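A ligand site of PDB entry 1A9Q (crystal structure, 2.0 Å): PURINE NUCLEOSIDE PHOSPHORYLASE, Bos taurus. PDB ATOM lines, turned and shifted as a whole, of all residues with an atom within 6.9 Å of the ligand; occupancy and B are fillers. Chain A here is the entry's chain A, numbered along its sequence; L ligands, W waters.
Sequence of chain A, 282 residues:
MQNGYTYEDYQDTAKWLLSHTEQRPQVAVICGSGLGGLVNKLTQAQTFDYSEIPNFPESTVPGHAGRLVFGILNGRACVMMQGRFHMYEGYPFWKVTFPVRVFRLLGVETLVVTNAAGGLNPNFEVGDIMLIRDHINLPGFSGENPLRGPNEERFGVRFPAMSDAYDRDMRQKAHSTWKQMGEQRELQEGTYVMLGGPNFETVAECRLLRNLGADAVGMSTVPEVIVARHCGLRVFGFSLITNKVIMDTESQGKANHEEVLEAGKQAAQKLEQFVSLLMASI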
ATOM      1  N   ALA A 116     -10.935 -27.454  20.303  1.00  0.00           N
ATOM      2  CA  ALA A 116      -9.805 -28.014  19.593  1.00  0.00           C
ATOM      3  C   ALA A 116      -9.174 -26.769  18.981  1.00  0.00           C
ATOM      4  O   ALA A 116      -9.885 -25.806  18.703  1.00  0.00           O
ATOM      5  CB  ALA A 116     -10.271 -28.949  18.503  1.00  0.00           C
ATOM      6  N   ALA A 117      -7.868 -26.755  18.795  1.00  0.00           N
ATOM      7  CA  ALA A 117      -7.223 -25.575  18.250  1.00  0.00           C
ATOM      8  C   ALA A 117      -5.980 -25.935  17.494  1.00  0.00           C
ATOM      9  O   ALA A 117      -5.400 -27.006  17.697  1.00  0.00           O
ATOM     10  CB  ALA A 117      -6.890 -24.607  19.375  1.00  0.00           C
ATOM     11  N   GLY A 118      -5.574 -25.045  16.600  1.00  0.00           N
ATOM     12  CA  GLY A 118      -4.363 -25.259  15.834  1.00  0.00           C
ATOM     13  C   GLY A 118      -3.267 -24.568  16.615  1.00  0.00           C
ATOM     14  O   GLY A 118      -3.481 -23.490  17.167  1.00  0.00           O
ATOM     15  N   GLY A 119      -2.094 -25.179  16.672  1.00  0.00           N
ATOM     16  CA  GLY A 119      -0.998 -24.578  17.402  1.00  0.00           C
ATOM     17  C   GLY A 119      -0.204 -23.588  16.567  1.00  0.00           C
ATOM     18  O   GLY A 119       0.246 -23.915  15.460  1.00  0.00           O
ATOM     19  N   TYR A 192      -5.674 -17.490  22.992  1.00  0.00           N
ATOM     20  CA  TYR A 192      -6.436 -18.126  21.940  1.00  0.00           C
ATOM     21  C   TYR A 192      -6.993 -17.010  21.054  1.00  0.00           C
ATOM     22  O   TYR A 192      -7.415 -15.963  21.538  1.00  0.00           O
ATOM     23  CB  TYR A 192      -7.573 -18.915  22.590  1.00  0.00           C
ATOM     24  CG  TYR A 192      -8.563 -19.512  21.627  1.00  0.00           C
ATOM     25  CD1 TYR A 192      -8.330 -20.740  21.038  1.00  0.00           C
ATOM     26  CD2 TYR A 192      -9.758 -18.848  21.339  1.00  0.00           C
ATOM     27  CE1 TYR A 192      -9.261 -21.321  20.188  1.00  0.00           C
ATOM     28  CE2 TYR A 192     -10.703 -19.410  20.497  1.00  0.00           C
ATOM     29  CZ  TYR A 192     -10.445 -20.648  19.931  1.00  0.00           C
ATOM     30  OH  TYR A 192     -11.379 -21.225  19.095  1.00  0.00           O
ATOM     31  N   LEU A 195     -11.343 -16.811  14.777  1.00  0.00           N
ATOM     32  CA  LEU A 195     -11.657 -16.246  13.475  1.00  0.00           C
ATOM     33  C   LEU A 195     -12.881 -17.029  13.007  1.00  0.00           C
ATOM     34  O   LEU A 195     -13.206 -18.058  13.605  1.00  0.00           O
ATOM     35  CB  LEU A 195     -10.477 -16.339  12.495  1.00  0.00           C
ATOM     36  CG  LEU A 195      -9.500 -17.517  12.554  1.00  0.00           C
ATOM     37  CD1 LEU A 195     -10.254 -18.826  12.346  1.00  0.00           C
ATOM     38  CD2 LEU A 195      -8.417 -17.322  11.488  1.00  0.00           C
ATOM     39  N   PRO A 198     -15.257 -21.419   7.664  1.00  0.00           N
ATOM     40  CA  PRO A 198     -14.836 -22.759   8.080  1.00  0.00           C
ATOM     41  C   PRO A 198     -13.545 -23.263   7.458  1.00  0.00           C
ATOM     42  O   PRO A 198     -13.068 -24.351   7.800  1.00  0.00           O
ATOM     43  CB  PRO A 198     -16.009 -23.619   7.622  1.00  0.00           C
ATOM     44  CG  PRO A 198     -16.384 -22.976   6.330  1.00  0.00           C
ATOM     45  CD  PRO A 198     -16.345 -21.496   6.684  1.00  0.00           C
ATOM     46  N   ASN A 199     -12.985 -22.512   6.525  1.00  0.00           N
ATOM     47  CA  ASN A 199     -11.753 -22.928   5.872  1.00  0.00           C
ATOM     48  C   ASN A 199     -10.576 -22.767   6.826  1.00  0.00           C
ATOM     49  O   ASN A 199     -10.666 -22.015   7.782  1.00  0.00           O
ATOM     50  CB  ASN A 199     -11.511 -22.110   4.594  1.00  0.00           C
ATOM     51  CG  ASN A 199     -11.184 -20.667   4.880  1.00  0.00           C
ATOM     52  OD1 ASN A 199     -12.072 -19.837   5.058  1.00  0.00           O
ATOM     53  ND2 ASN A 199      -9.900 -20.361   4.961  1.00  0.00           N
ATOM     54  N   PHE A 200      -9.514 -23.522   6.576  1.00  0.00           N
ATOM     55  CA  PHE A 200      -8.306 -23.446   7.380  1.00  0.00           C
ATOM     56  C   PHE A 200      -7.423 -22.296   6.836  1.00  0.00           C
ATOM     57  O   PHE A 200      -7.501 -21.932   5.665  1.00  0.00           O
ATOM     58  CB  PHE A 200      -7.539 -24.778   7.368  1.00  0.00           C
ATOM     59  CG  PHE A 200      -8.199 -25.872   8.187  1.00  0.00           C
ATOM     60  CD1 PHE A 200      -8.330 -25.750   9.573  1.00  0.00           C
ATOM     61  CD2 PHE A 200      -8.652 -27.048   7.580  1.00  0.00           C
ATOM     62  CE1 PHE A 200      -8.913 -26.769  10.335  1.00  0.00           C
ATOM     63  CE2 PHE A 200      -9.229 -28.075   8.346  1.00  0.00           C
ATOM     64  CZ  PHE A 200      -9.360 -27.929   9.726  1.00  0.00           C
ATOM     65  N   GLU A 201      -6.549 -21.768   7.695  1.00  0.00           N
ATOM     66  CA  GLU A 201      -5.694 -20.642   7.354  1.00  0.00           C
ATOM     67  C   GLU A 201      -4.616 -20.890   6.327  1.00  0.00           C
ATOM     68  O   GLU A 201      -4.233 -22.027   6.069  1.00  0.00           O
ATOM     69  CB  GLU A 201      -5.039 -20.077   8.611  1.00  0.00           C
ATOM     70  CG  GLU A 201      -6.005 -19.638   9.692  1.00  0.00           C
ATOM     71  CD  GLU A 201      -6.654 -20.814  10.401  1.00  0.00           C
ATOM     72  OE1 GLU A 201      -5.958 -21.815  10.649  1.00  0.00           O
ATOM     73  OE2 GLU A 201      -7.857 -20.744  10.714  1.00  0.00           O
ATOM     74  N   CYS A 206      -1.343 -17.393   9.079  1.00  0.00           N
ATOM     75  CA  CYS A 206      -0.805 -18.003  10.285  1.00  0.00           C
ATOM     76  C   CYS A 206       0.377 -17.225  10.843  1.00  0.00           C
ATOM     77  O   CYS A 206       0.559 -17.135  12.067  1.00  0.00           O
ATOM     78  CB  CYS A 206      -0.380 -19.447  10.017  1.00  0.00           C
ATOM     79  SG  CYS A 206      -1.719 -20.616   9.962  1.00  0.00           S
ATOM     80  N   VAL A 217      -5.219 -21.049  17.463  1.00  0.00           N
ATOM     81  CA  VAL A 217      -6.288 -20.507  16.630  1.00  0.00           C
ATOM     82  C   VAL A 217      -7.470 -21.464  16.566  1.00  0.00           C
ATOM     83  O   VAL A 217      -7.286 -22.680  16.533  1.00  0.00           O
ATOM     84  CB  VAL A 217      -5.762 -20.182  15.200  1.00  0.00           C
ATOM     85  CG1 VAL A 217      -5.114 -21.401  14.574  1.00  0.00           C
ATOM     86  CG2 VAL A 217      -6.884 -19.640  14.310  1.00  0.00           C
ATOM     87  N   GLY A 218      -8.680 -20.909  16.569  1.00  0.00           N
ATOM     88  CA  GLY A 218      -9.878 -21.730  16.508  1.00  0.00           C
ATOM     89  C   GLY A 218     -11.056 -20.947  15.981  1.00  0.00           C
ATOM     90  O   GLY A 218     -10.962 -19.752  15.728  1.00  0.00           O
ATOM     91  N   MET A 219     -12.202 -21.626  15.847  1.00  0.00           N
ATOM     92  CA  MET A 219     -13.396 -20.995  15.306  1.00  0.00           C
ATOM     93  C   MET A 219     -14.567 -20.937  16.282  1.00  0.00           C
ATOM     94  O   MET A 219     -15.744 -20.940  15.855  1.00  0.00           O
ATOM     95  CB  MET A 219     -13.827 -21.756  14.033  1.00  0.00           C
ATOM     96  CG  MET A 219     -12.734 -21.909  12.983  1.00  0.00           C
ATOM     97  SD  MET A 219     -13.177 -23.092  11.690  1.00  0.00           S
ATOM     98  CE  MET A 219     -11.589 -23.202  10.776  1.00  0.00           C
ATOM     99  N   LEU A 240      -7.439 -28.080  23.121  1.00  0.00           N
ATOM    100  CA  LEU A 240      -6.690 -29.295  22.862  1.00  0.00           C
ATOM    101  C   LEU A 240      -5.976 -28.970  21.557  1.00  0.00           C
ATOM    102  O   LEU A 240      -6.624 -28.646  20.563  1.00  0.00           O
ATOM    103  CB  LEU A 240      -7.637 -30.483  22.629  1.00  0.00           C
ATOM    104  CG  LEU A 240      -6.923 -31.755  22.160  1.00  0.00           C
ATOM    105  CD1 LEU A 240      -5.954 -32.250  23.236  1.00  0.00           C
ATOM    106  CD2 LEU A 240      -7.934 -32.837  21.853  1.00  0.00           C
ATOM    107  N   THR A 242      -4.829 -29.833  18.517  1.00  0.00           N
ATOM    108  CA  THR A 242      -5.071 -30.954  17.611  1.00  0.00           C
ATOM    109  C   THR A 242      -4.141 -31.069  16.417  1.00  0.00           C
ATOM    110  O   THR A 242      -4.108 -32.097  15.750  1.00  0.00           O
ATOM    111  CB  THR A 242      -6.556 -30.976  17.136  1.00  0.00           C
ATOM    112  OG1 THR A 242      -6.907 -29.702  16.574  1.00  0.00           O
ATOM    113  CG2 THR A 242      -7.492 -31.256  18.296  1.00  0.00           C
ATOM    114  N   ASN A 243      -3.382 -30.015  16.142  1.00  0.00           N
ATOM    115  CA  ASN A 243      -2.470 -30.004  15.021  1.00  0.00           C
ATOM    116  C   ASN A 243      -1.616 -28.764  15.084  1.00  0.00           C
ATOM    117  O   ASN A 243      -1.951 -27.809  15.778  1.00  0.00           O
ATOM    118  CB  ASN A 243      -3.250 -30.016  13.686  1.00  0.00           C
ATOM    119  CG  ASN A 243      -4.124 -28.774  13.505  1.00  0.00           C
ATOM    120  OD1 ASN A 243      -5.124 -28.599  14.208  1.00  0.00           O
ATOM    121  ND2 ASN A 243      -3.778 -27.933  12.544  1.00  0.00           N
ATOM    122  N   LYS A 244      -0.484 -28.798  14.407  1.00  0.00           N
ATOM    123  CA  LYS A 244       0.422 -27.658  14.337  1.00  0.00           C
ATOM    124  C   LYS A 244       0.203 -27.055  12.955  1.00  0.00           C
ATOM    125  O   LYS A 244       0.174 -27.769  11.962  1.00  0.00           O
ATOM    126  CB  LYS A 244       1.871 -28.119  14.519  1.00  0.00           C
ATOM    127  CG  LYS A 244       2.129 -28.751  15.887  1.00  0.00           C
ATOM    128  CD  LYS A 244       3.496 -29.450  15.952  1.00  0.00           C
ATOM    129  CE  LYS A 244       4.666 -28.478  15.949  1.00  0.00           C
ATOM    130  NZ  LYS A 244       5.962 -29.201  16.111  1.00  0.00           N
ATOM    131  N   VAL A 245      -0.007 -25.735  12.908  1.00  0.00           N
ATOM    132  CA  VAL A 245      -0.267 -25.056  11.646  1.00  0.00           C
ATOM    133  C   VAL A 245       0.939 -24.941  10.697  1.00  0.00           C
ATOM    134  O   VAL A 245       2.059 -24.702  11.121  1.00  0.00           O
ATOM    135  CB  VAL A 245      -0.895 -23.651  11.880  1.00  0.00           C
ATOM    136  CG1 VAL A 245      -2.142 -23.771  12.738  1.00  0.00           C
ATOM    137  CG2 VAL A 245       0.118 -22.724  12.523  1.00  0.00           C
ATOM    138  N   ILE A 246       0.672 -25.128   9.405  1.00  0.00           N
ATOM    139  CA  ILE A 246       1.687 -25.042   8.362  1.00  0.00           C
ATOM    140  C   ILE A 246       2.114 -23.574   8.235  1.00  0.00           C
ATOM    141  O   ILE A 246       1.289 -22.718   7.917  1.00  0.00           O
ATOM    142  CB  ILE A 246       1.103 -25.478   6.971  1.00  0.00           C
ATOM    143  CG1 ILE A 246       0.439 -26.860   7.043  1.00  0.00           C
ATOM    144  CG2 ILE A 246       2.190 -25.439   5.911  1.00  0.00           C
ATOM    145  CD1 ILE A 246       1.405 -28.022   7.096  1.00  0.00           C
ATOM    146  N   ALA A 255      -3.461 -28.927   6.922  1.00  0.00           N
ATOM    147  CA  ALA A 255      -4.430 -29.234   7.962  1.00  0.00           C
ATOM    148  C   ALA A 255      -5.686 -29.848   7.358  1.00  0.00           C
ATOM    149  O   ALA A 255      -6.198 -29.376   6.338  1.00  0.00           O
ATOM    150  CB  ALA A 255      -4.790 -27.970   8.731  1.00  0.00           C
ATOM    151  N   VAL A 260      -7.562 -33.633  13.012  1.00  0.00           N
ATOM    152  CA  VAL A 260      -8.063 -33.091  14.266  1.00  0.00           C
ATOM    153  C   VAL A 260      -8.954 -34.072  15.016  1.00  0.00           C
ATOM    154  O   VAL A 260      -8.928 -34.127  16.247  1.00  0.00           O
ATOM    155  CB  VAL A 260      -8.773 -31.716  14.098  1.00  0.00           C
ATOM    156  CG1 VAL A 260      -7.947 -30.800  13.194  1.00  0.00           C
ATOM    157  CG2 VAL A 260     -10.183 -31.867  13.593  1.00  0.00           C
HETATM  158  N1  LIG L   1      -7.201 -23.687  12.320  1.00  0.00           N
HETATM  159  C1  LIG L   1      -8.409 -23.197  12.710  1.00  0.00           C
HETATM  160  N2  LIG L   1      -9.205 -23.827  13.541  1.00  0.00           N
HETATM  161  C2  LIG L   1      -8.686 -24.994  13.961  1.00  0.00           C
HETATM  162  C3  LIG L   1      -7.482 -25.538  13.608  1.00  0.00           C
HETATM  163  C4  LIG L   1      -6.633 -24.871  12.710  1.00  0.00           C
HETATM  164  O1  LIG L   1      -5.519 -25.171  12.277  1.00  0.00           O
HETATM  165  N3  LIG L   1      -7.346 -26.731  14.272  1.00  0.00           N
HETATM  166  C5  LIG L   1      -8.450 -26.896  15.025  1.00  0.00           C
HETATM  167  N4  LIG L   1      -9.307 -25.838  14.853  1.00  0.00           N
HETATM  168  O   HOH W   1      -4.632 -24.067   9.576  1.00  0.00           O
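A nitrogen (N1) of the ligand sits at hydrogen-bond distance from the side-chain carboxylate of Glu 201 (2.8 Å). OD1 of Asn 243 lies within hydrogen-bond range of N3 of the ligand (2.9 Å). The backbone NH (N) of Gly 118 sits close to a nitrogen (N3) of the ligand.
OG1 of Thr 242 is in hydrogen-bond range of OD1 of Asn 243, at 3.2 Å. O of Asn 243 sits at hydrogen-bond distance from N of Gly 119 (2.8 Å). The backbone NH of Gly 118 sits at hydrogen-bond distance from the backbone carbonyl oxygen of Val 217, 2.9 Å away. The backbone NH of Thr 242 is in hydrogen-bond range of the backbone carbonyl oxygen of Ala 117 (3.0 Å). O of Leu 240 lies within hydrogen-bond range of N of Ala 117, at 2.9 Å. The backbone NH of Val 245 sits at hydrogen-bond distance from the backbone carbonyl oxygen of Gly 119 (3.1 Å). The backbone carbonyl oxygen (O) of Gly 218 lies within hydrogen-bond range of the backbone NH (N) of Leu 195, 3.1 Å away. N of Met 219 sits at hydrogen-bond distance from OH of Tyr 192 (3.4 Å).
Ala 116 touches the ligand (O to N4, 3.9 Å). Ala 117 touches the ligand (C to N3, 3.6 Å). CD1 of Phe 200 touches N1 of the ligand (3.6 Å). O of Val 217 touches C2 of the ligand (3.7 Å). CA of Gly 218 touches N2 of the ligand (3.7 Å). Met 219 touches the ligand (CE to N2, 3.7 Å). Thr 242 touches the ligand (OG1 to C5, 3.6 Å). Val 245 touches the ligand. Hydrophobic or aromatic side chains within 4 Å of the ligand: Phe 200, Val 217, Met 219 and Val 245. Within 4 Å of the ligand: Ala 116, Ala 117, Gly 118, Phe 200, Glu 201, Val 217, Gly 218, Met 219, Thr 242, Asn 243 and Val 245.
Water W1 lies within hydrogen-bond range of the side-chain carboxylate (OE1) of Glu 201 (2.8 Å) and an oxygen (O1) of the ligand (3.0 Å).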
